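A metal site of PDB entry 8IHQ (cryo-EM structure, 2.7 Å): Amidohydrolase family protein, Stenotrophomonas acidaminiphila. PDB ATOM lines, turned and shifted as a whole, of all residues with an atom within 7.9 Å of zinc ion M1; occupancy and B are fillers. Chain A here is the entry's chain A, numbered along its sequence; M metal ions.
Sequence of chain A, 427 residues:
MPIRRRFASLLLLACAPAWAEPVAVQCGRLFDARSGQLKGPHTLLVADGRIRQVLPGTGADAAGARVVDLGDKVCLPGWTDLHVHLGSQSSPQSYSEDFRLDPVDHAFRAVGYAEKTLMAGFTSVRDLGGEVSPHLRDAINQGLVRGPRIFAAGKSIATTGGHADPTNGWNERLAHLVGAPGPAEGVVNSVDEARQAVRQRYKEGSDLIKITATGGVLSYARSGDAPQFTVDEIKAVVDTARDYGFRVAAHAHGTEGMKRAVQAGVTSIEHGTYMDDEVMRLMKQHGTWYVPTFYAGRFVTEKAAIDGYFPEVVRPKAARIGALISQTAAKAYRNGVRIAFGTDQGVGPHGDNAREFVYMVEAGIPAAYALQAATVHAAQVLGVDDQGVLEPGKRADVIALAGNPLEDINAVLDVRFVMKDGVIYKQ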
ATOM      1  N   HIS A  83       5.083  24.560  33.406  1.00  0.00           N
ATOM      2  CA  HIS A  83       4.791  23.824  32.187  1.00  0.00           C
ATOM      3  C   HIS A  83       3.378  23.239  32.319  1.00  0.00           C
ATOM      4  O   HIS A  83       3.193  22.222  32.973  1.00  0.00           O
ATOM      5  CB  HIS A  83       5.817  22.727  31.946  1.00  0.00           C
ATOM      6  CG  HIS A  83       5.875  22.245  30.531  1.00  0.00           C
ATOM      7  ND1 HIS A  83       6.966  21.582  30.021  1.00  0.00           N
ATOM      8  CD2 HIS A  83       4.981  22.327  29.523  1.00  0.00           C
ATOM      9  CE1 HIS A  83       6.740  21.276  28.753  1.00  0.00           C
ATOM     10  NE2 HIS A  83       5.534  21.710  28.434  1.00  0.00           N
ATOM     11  N   VAL A  84       2.403  23.920  31.701  1.00  0.00           N
ATOM     12  CA  VAL A  84       1.029  23.448  31.657  1.00  0.00           C
ATOM     13  C   VAL A  84       0.467  23.705  30.264  1.00  0.00           C
ATOM     14  O   VAL A  84       0.998  24.491  29.490  1.00  0.00           O
ATOM     15  CB  VAL A  84       0.111  24.129  32.721  1.00  0.00           C
ATOM     16  CG1 VAL A  84       0.718  24.020  34.113  1.00  0.00           C
ATOM     17  CG2 VAL A  84      -0.134  25.574  32.354  1.00  0.00           C
ATOM     18  N   HIS A  85      -0.644  23.015  29.968  1.00  0.00           N
ATOM     19  CA  HIS A  85      -1.417  23.235  28.738  1.00  0.00           C
ATOM     20  C   HIS A  85      -2.882  23.283  29.161  1.00  0.00           C
ATOM     21  O   HIS A  85      -3.565  22.266  29.177  1.00  0.00           O
ATOM     22  CB  HIS A  85      -1.153  22.141  27.704  1.00  0.00           C
ATOM     23  CG  HIS A  85       0.279  22.002  27.331  1.00  0.00           C
ATOM     24  ND1 HIS A  85       0.873  22.778  26.347  1.00  0.00           N
ATOM     25  CD2 HIS A  85       1.254  21.191  27.800  1.00  0.00           C
ATOM     26  CE1 HIS A  85       2.140  22.445  26.234  1.00  0.00           C
ATOM     27  NE2 HIS A  85       2.406  21.477  27.100  1.00  0.00           N
ATOM     28  N   ASP A 127       2.019  28.817  30.546  1.00  0.00           N
ATOM     29  CA  ASP A 127       1.469  27.983  29.497  1.00  0.00           C
ATOM     30  C   ASP A 127       2.423  27.970  28.305  1.00  0.00           C
ATOM     31  O   ASP A 127       2.833  29.032  27.813  1.00  0.00           O
ATOM     32  CB  ASP A 127       0.094  28.505  29.069  1.00  0.00           C
ATOM     33  CG  ASP A 127      -0.661  27.517  28.215  1.00  0.00           C
ATOM     34  OD1 ASP A 127      -0.313  27.370  27.021  1.00  0.00           O
ATOM     35  OD2 ASP A 127      -1.601  26.880  28.727  1.00  0.00           O
ATOM     36  N   LEU A 128       2.778  26.774  27.844  1.00  0.00           N
ATOM     37  CA  LEU A 128       3.836  26.586  26.861  1.00  0.00           C
ATOM     38  C   LEU A 128       3.275  26.017  25.560  1.00  0.00           C
ATOM     39  O   LEU A 128       3.849  25.111  24.955  1.00  0.00           O
ATOM     40  CB  LEU A 128       4.929  25.672  27.405  1.00  0.00           C
ATOM     41  CG  LEU A 128       5.961  26.323  28.342  1.00  0.00           C
ATOM     42  CD1 LEU A 128       7.123  25.376  28.577  1.00  0.00           C
ATOM     43  CD2 LEU A 128       6.446  27.651  27.796  1.00  0.00           C
ATOM     44  N   GLY A 129       2.144  26.544  25.106  1.00  0.00           N
ATOM     45  CA  GLY A 129       1.556  26.114  23.852  1.00  0.00           C
ATOM     46  C   GLY A 129       0.043  26.119  23.850  1.00  0.00           C
ATOM     47  O   GLY A 129      -0.584  25.597  24.768  1.00  0.00           O
ATOM     48  N   HIS A 163       7.850  18.681  15.825  1.00  0.00           N
ATOM     49  CA  HIS A 163       6.977  18.246  16.900  1.00  0.00           C
ATOM     50  C   HIS A 163       5.736  19.118  17.026  1.00  0.00           C
ATOM     51  O   HIS A 163       4.664  18.623  17.375  1.00  0.00           O
ATOM     52  CB  HIS A 163       7.746  18.215  18.224  1.00  0.00           C
ATOM     53  CG  HIS A 163       6.942  17.717  19.388  1.00  0.00           C
ATOM     54  ND1 HIS A 163       6.338  16.478  19.398  1.00  0.00           N
ATOM     55  CD2 HIS A 163       6.650  18.283  20.576  1.00  0.00           C
ATOM     56  CE1 HIS A 163       5.700  16.307  20.532  1.00  0.00           C
ATOM     57  NE2 HIS A 163       5.871  17.394  21.267  1.00  0.00           N
ATOM     58  N   KCX A 210       8.312  29.738  22.647  1.00  0.00           N
ATOM     59  CA  KCX A 210       8.465  28.290  22.800  1.00  0.00           C
ATOM     60  CB  KCX A 210       7.153  27.667  23.297  1.00  0.00           C
ATOM     61  CG  KCX A 210       7.307  26.573  24.343  1.00  0.00           C
ATOM     62  CD  KCX A 210       8.159  25.420  23.859  1.00  0.00           C
ATOM     63  CE  KCX A 210       8.052  24.231  24.788  1.00  0.00           C
ATOM     64  NZ  KCX A 210       6.706  23.607  24.699  1.00  0.00           N
ATOM     65  C   KCX A 210       8.889  27.638  21.492  1.00  0.00           C
ATOM     66  O   KCX A 210       8.209  27.787  20.466  1.00  0.00           O
ATOM     67  CX  KCX A 210       6.514  22.367  25.150  1.00  0.00           C
ATOM     68  OQ1 KCX A 210       5.381  21.856  25.068  1.00  0.00           O
ATOM     69  OQ2 KCX A 210       7.451  21.734  25.645  1.00  0.00           O
ATOM     70  N   THR A 212      10.424  23.847  19.675  1.00  0.00           N
ATOM     71  CA  THR A 212      10.675  22.412  19.802  1.00  0.00           C
ATOM     72  C   THR A 212      12.040  22.120  19.183  1.00  0.00           C
ATOM     73  O   THR A 212      12.183  22.122  17.953  1.00  0.00           O
ATOM     74  CB  THR A 212       9.579  21.604  19.117  1.00  0.00           C
ATOM     75  OG1 THR A 212       9.432  22.038  17.763  1.00  0.00           O
ATOM     76  CG2 THR A 212       8.254  21.769  19.845  1.00  0.00           C
ATOM     77  N   LEU A 218       4.347  12.613  21.652  1.00  0.00           N
ATOM     78  CA  LEU A 218       2.910  12.618  21.384  1.00  0.00           C
ATOM     79  C   LEU A 218       2.559  13.115  19.987  1.00  0.00           C
ATOM     80  O   LEU A 218       1.385  13.105  19.625  1.00  0.00           O
ATOM     81  CB  LEU A 218       2.193  13.460  22.441  1.00  0.00           C
ATOM     82  CG  LEU A 218       2.101  12.851  23.838  1.00  0.00           C
ATOM     83  CD1 LEU A 218       1.452  13.825  24.806  1.00  0.00           C
ATOM     84  CD2 LEU A 218       1.347  11.539  23.817  1.00  0.00           C
ATOM     85  N   HIS A 251      11.738  22.601  24.122  1.00  0.00           N
ATOM     86  CA  HIS A 251      11.406  21.185  24.378  1.00  0.00           C
ATOM     87  C   HIS A 251      12.501  20.329  23.732  1.00  0.00           C
ATOM     88  O   HIS A 251      12.756  20.532  22.542  1.00  0.00           O
ATOM     89  CB  HIS A 251      10.021  20.889  23.783  1.00  0.00           C
ATOM     90  CG  HIS A 251       9.840  19.497  23.276  1.00  0.00           C
ATOM     91  ND1 HIS A 251       8.959  18.610  23.875  1.00  0.00           N
ATOM     92  CD2 HIS A 251      10.379  18.847  22.223  1.00  0.00           C
ATOM     93  CE1 HIS A 251       8.993  17.472  23.219  1.00  0.00           C
ATOM     94  NE2 HIS A 251       9.855  17.585  22.213  1.00  0.00           N
ATOM     95  N   GLU A 270      12.990  21.888  28.524  1.00  0.00           N
ATOM     96  CA  GLU A 270      11.731  21.317  28.993  1.00  0.00           C
ATOM     97  C   GLU A 270      11.831  19.824  29.298  1.00  0.00           C
ATOM     98  O   GLU A 270      11.090  19.328  30.156  1.00  0.00           O
ATOM     99  CB  GLU A 270      10.616  21.556  27.967  1.00  0.00           C
ATOM    100  CG  GLU A 270      10.111  22.989  27.908  1.00  0.00           C
ATOM    101  CD  GLU A 270      10.190  23.711  29.243  1.00  0.00           C
ATOM    102  OE1 GLU A 270       9.623  23.210  30.240  1.00  0.00           O
ATOM    103  OE2 GLU A 270      10.818  24.788  29.296  1.00  0.00           O
ATOM    104  N   HIS A 271      12.694  19.086  28.613  1.00  0.00           N
ATOM    105  CA  HIS A 271      12.951  17.696  28.949  1.00  0.00           C
ATOM    106  C   HIS A 271      14.422  17.407  28.744  1.00  0.00           C
ATOM    107  O   HIS A 271      15.126  18.114  28.021  1.00  0.00           O
ATOM    108  CB  HIS A 271      12.084  16.735  28.116  1.00  0.00           C
ATOM    109  CG  HIS A 271      10.666  17.167  27.948  1.00  0.00           C
ATOM    110  ND1 HIS A 271       9.724  17.053  28.942  1.00  0.00           N
ATOM    111  CD2 HIS A 271      10.020  17.723  26.889  1.00  0.00           C
ATOM    112  CE1 HIS A 271       8.563  17.509  28.515  1.00  0.00           C
ATOM    113  NE2 HIS A 271       8.723  17.925  27.269  1.00  0.00           N
ATOM    114  N   THR A 293       9.624  17.418  34.681  1.00  0.00           N
ATOM    115  CA  THR A 293       8.269  16.945  34.350  1.00  0.00           C
ATOM    116  C   THR A 293       8.172  15.424  34.498  1.00  0.00           C
ATOM    117  O   THR A 293       8.005  14.678  33.538  1.00  0.00           O
ATOM    118  CB  THR A 293       7.846  17.377  32.940  1.00  0.00           C
ATOM    119  OG1 THR A 293       8.510  16.561  31.962  1.00  0.00           O
ATOM    120  CG2 THR A 293       8.171  18.843  32.687  1.00  0.00           C
ATOM    121  N   ALA A 296       4.432  13.856  33.422  1.00  0.00           N
ATOM    122  CA  ALA A 296       4.136  13.523  32.029  1.00  0.00           C
ATOM    123  C   ALA A 296       4.771  12.195  31.629  1.00  0.00           C
ATOM    124  O   ALA A 296       4.141  11.392  30.938  1.00  0.00           O
ATOM    125  CB  ALA A 296       4.611  14.645  31.111  1.00  0.00           C
ATOM    126  N   THR A 343       5.134  20.556  35.375  1.00  0.00           N
ATOM    127  CA  THR A 343       4.371  19.314  35.360  1.00  0.00           C
ATOM    128  C   THR A 343       4.011  18.811  33.973  1.00  0.00           C
ATOM    129  O   THR A 343       3.806  17.605  33.818  1.00  0.00           O
ATOM    130  CB  THR A 343       3.070  19.482  36.159  1.00  0.00           C
ATOM    131  OG1 THR A 343       2.400  20.677  35.743  1.00  0.00           O
ATOM    132  CG2 THR A 343       3.344  19.552  37.642  1.00  0.00           C
ATOM    133  N   ASP A 344       3.901  19.694  32.978  1.00  0.00           N
ATOM    134  CA  ASP A 344       3.405  19.342  31.646  1.00  0.00           C
ATOM    135  C   ASP A 344       1.968  18.827  31.714  1.00  0.00           C
ATOM    136  O   ASP A 344       1.598  17.852  31.059  1.00  0.00           O
ATOM    137  CB  ASP A 344       4.313  18.315  30.959  1.00  0.00           C
ATOM    138  CG  ASP A 344       4.141  18.309  29.453  1.00  0.00           C
ATOM    139  OD1 ASP A 344       3.345  19.110  28.935  1.00  0.00           O
ATOM    140  OD2 ASP A 344       4.814  17.491  28.777  1.00  0.00           O
ATOM    141  N   GLN A 345       1.145  19.489  32.526  1.00  0.00           N
ATOM    142  CA  GLN A 345      -0.260  19.120  32.605  1.00  0.00           C
ATOM    143  C   GLN A 345      -0.968  19.473  31.298  1.00  0.00           C
ATOM    144  O   GLN A 345      -0.542  20.336  30.535  1.00  0.00           O
ATOM    145  CB  GLN A 345      -0.949  19.820  33.784  1.00  0.00           C
ATOM    146  CG  GLN A 345      -0.382  19.431  35.131  1.00  0.00           C
ATOM    147  CD  GLN A 345      -0.662  17.998  35.525  1.00  0.00           C
ATOM    148  OE1 GLN A 345      -1.651  17.703  36.200  1.00  0.00           O
ATOM    149  NE2 GLN A 345       0.207  17.083  35.112  1.00  0.00           N
ATOM    150  N   VAL A 347      -1.288  16.617  29.506  1.00  0.00           N
ATOM    151  CA  VAL A 347      -1.150  15.171  29.421  1.00  0.00           C
ATOM    152  C   VAL A 347      -1.841  14.509  30.620  1.00  0.00           C
ATOM    153  O   VAL A 347      -2.720  13.656  30.470  1.00  0.00           O
ATOM    154  CB  VAL A 347       0.327  14.766  29.331  1.00  0.00           C
ATOM    155  CG1 VAL A 347       0.467  13.291  29.037  1.00  0.00           C
ATOM    156  CG2 VAL A 347       1.038  15.588  28.270  1.00  0.00           C
HETATM  157 ZN    ZN M   1       4.526  20.731  26.616  1.00  0.00          ZN
HETATM  158 ZN    ZN M   2       7.721  19.054  25.523  1.00  0.00          ZN
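The backbone carbonyl oxygen of His 83 lies within hydrogen-bond range of the backbone NH of Asp 344 (2.6 Å).
The backbone NH (N) of His 85 sits at hydrogen-bond distance from the backbone carbonyl oxygen (O) of Gln 345, 2.7 Å away.
OE1 of Glu 270 lies within hydrogen-bond range of ND1 of His 83 (3.1 Å).
NE2 of His 85 sits close to OD1 of Asp 344.
The backbone carbonyl oxygen of Leu 128 lies within hydrogen-bond range of NZ of KCX 210, 3.2 Å away.
The backbone carbonyl oxygen (O) of His 83 sits at hydrogen-bond distance from the side-chain hydroxyl (OG1) of Thr 343 (3.3 Å).
The backbone carbonyl oxygen (O) of His 83 is in hydrogen-bond range of the backbone NH (N) of Gln 345 (3.4 Å).
Merely in contact with zinc ion M1: Asp 344.
Four residues have an atom within 4 Å of zinc ion M1: His 83, His 85, KCX 210 and Asp 344.
The nearest printed residue that does not touch zinc ion M1 is Leu 128 (4.7 Å).
OQ1 of KCX 210 binds zinc ion M1 (2.1 Å).
Zinc ion M1 is bound by NE2 of His 83.
NE2 of His 85 is bound to zinc ion M1, at 2.3 Å.
Zinc ion M1 has three donor atoms within binding distance.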
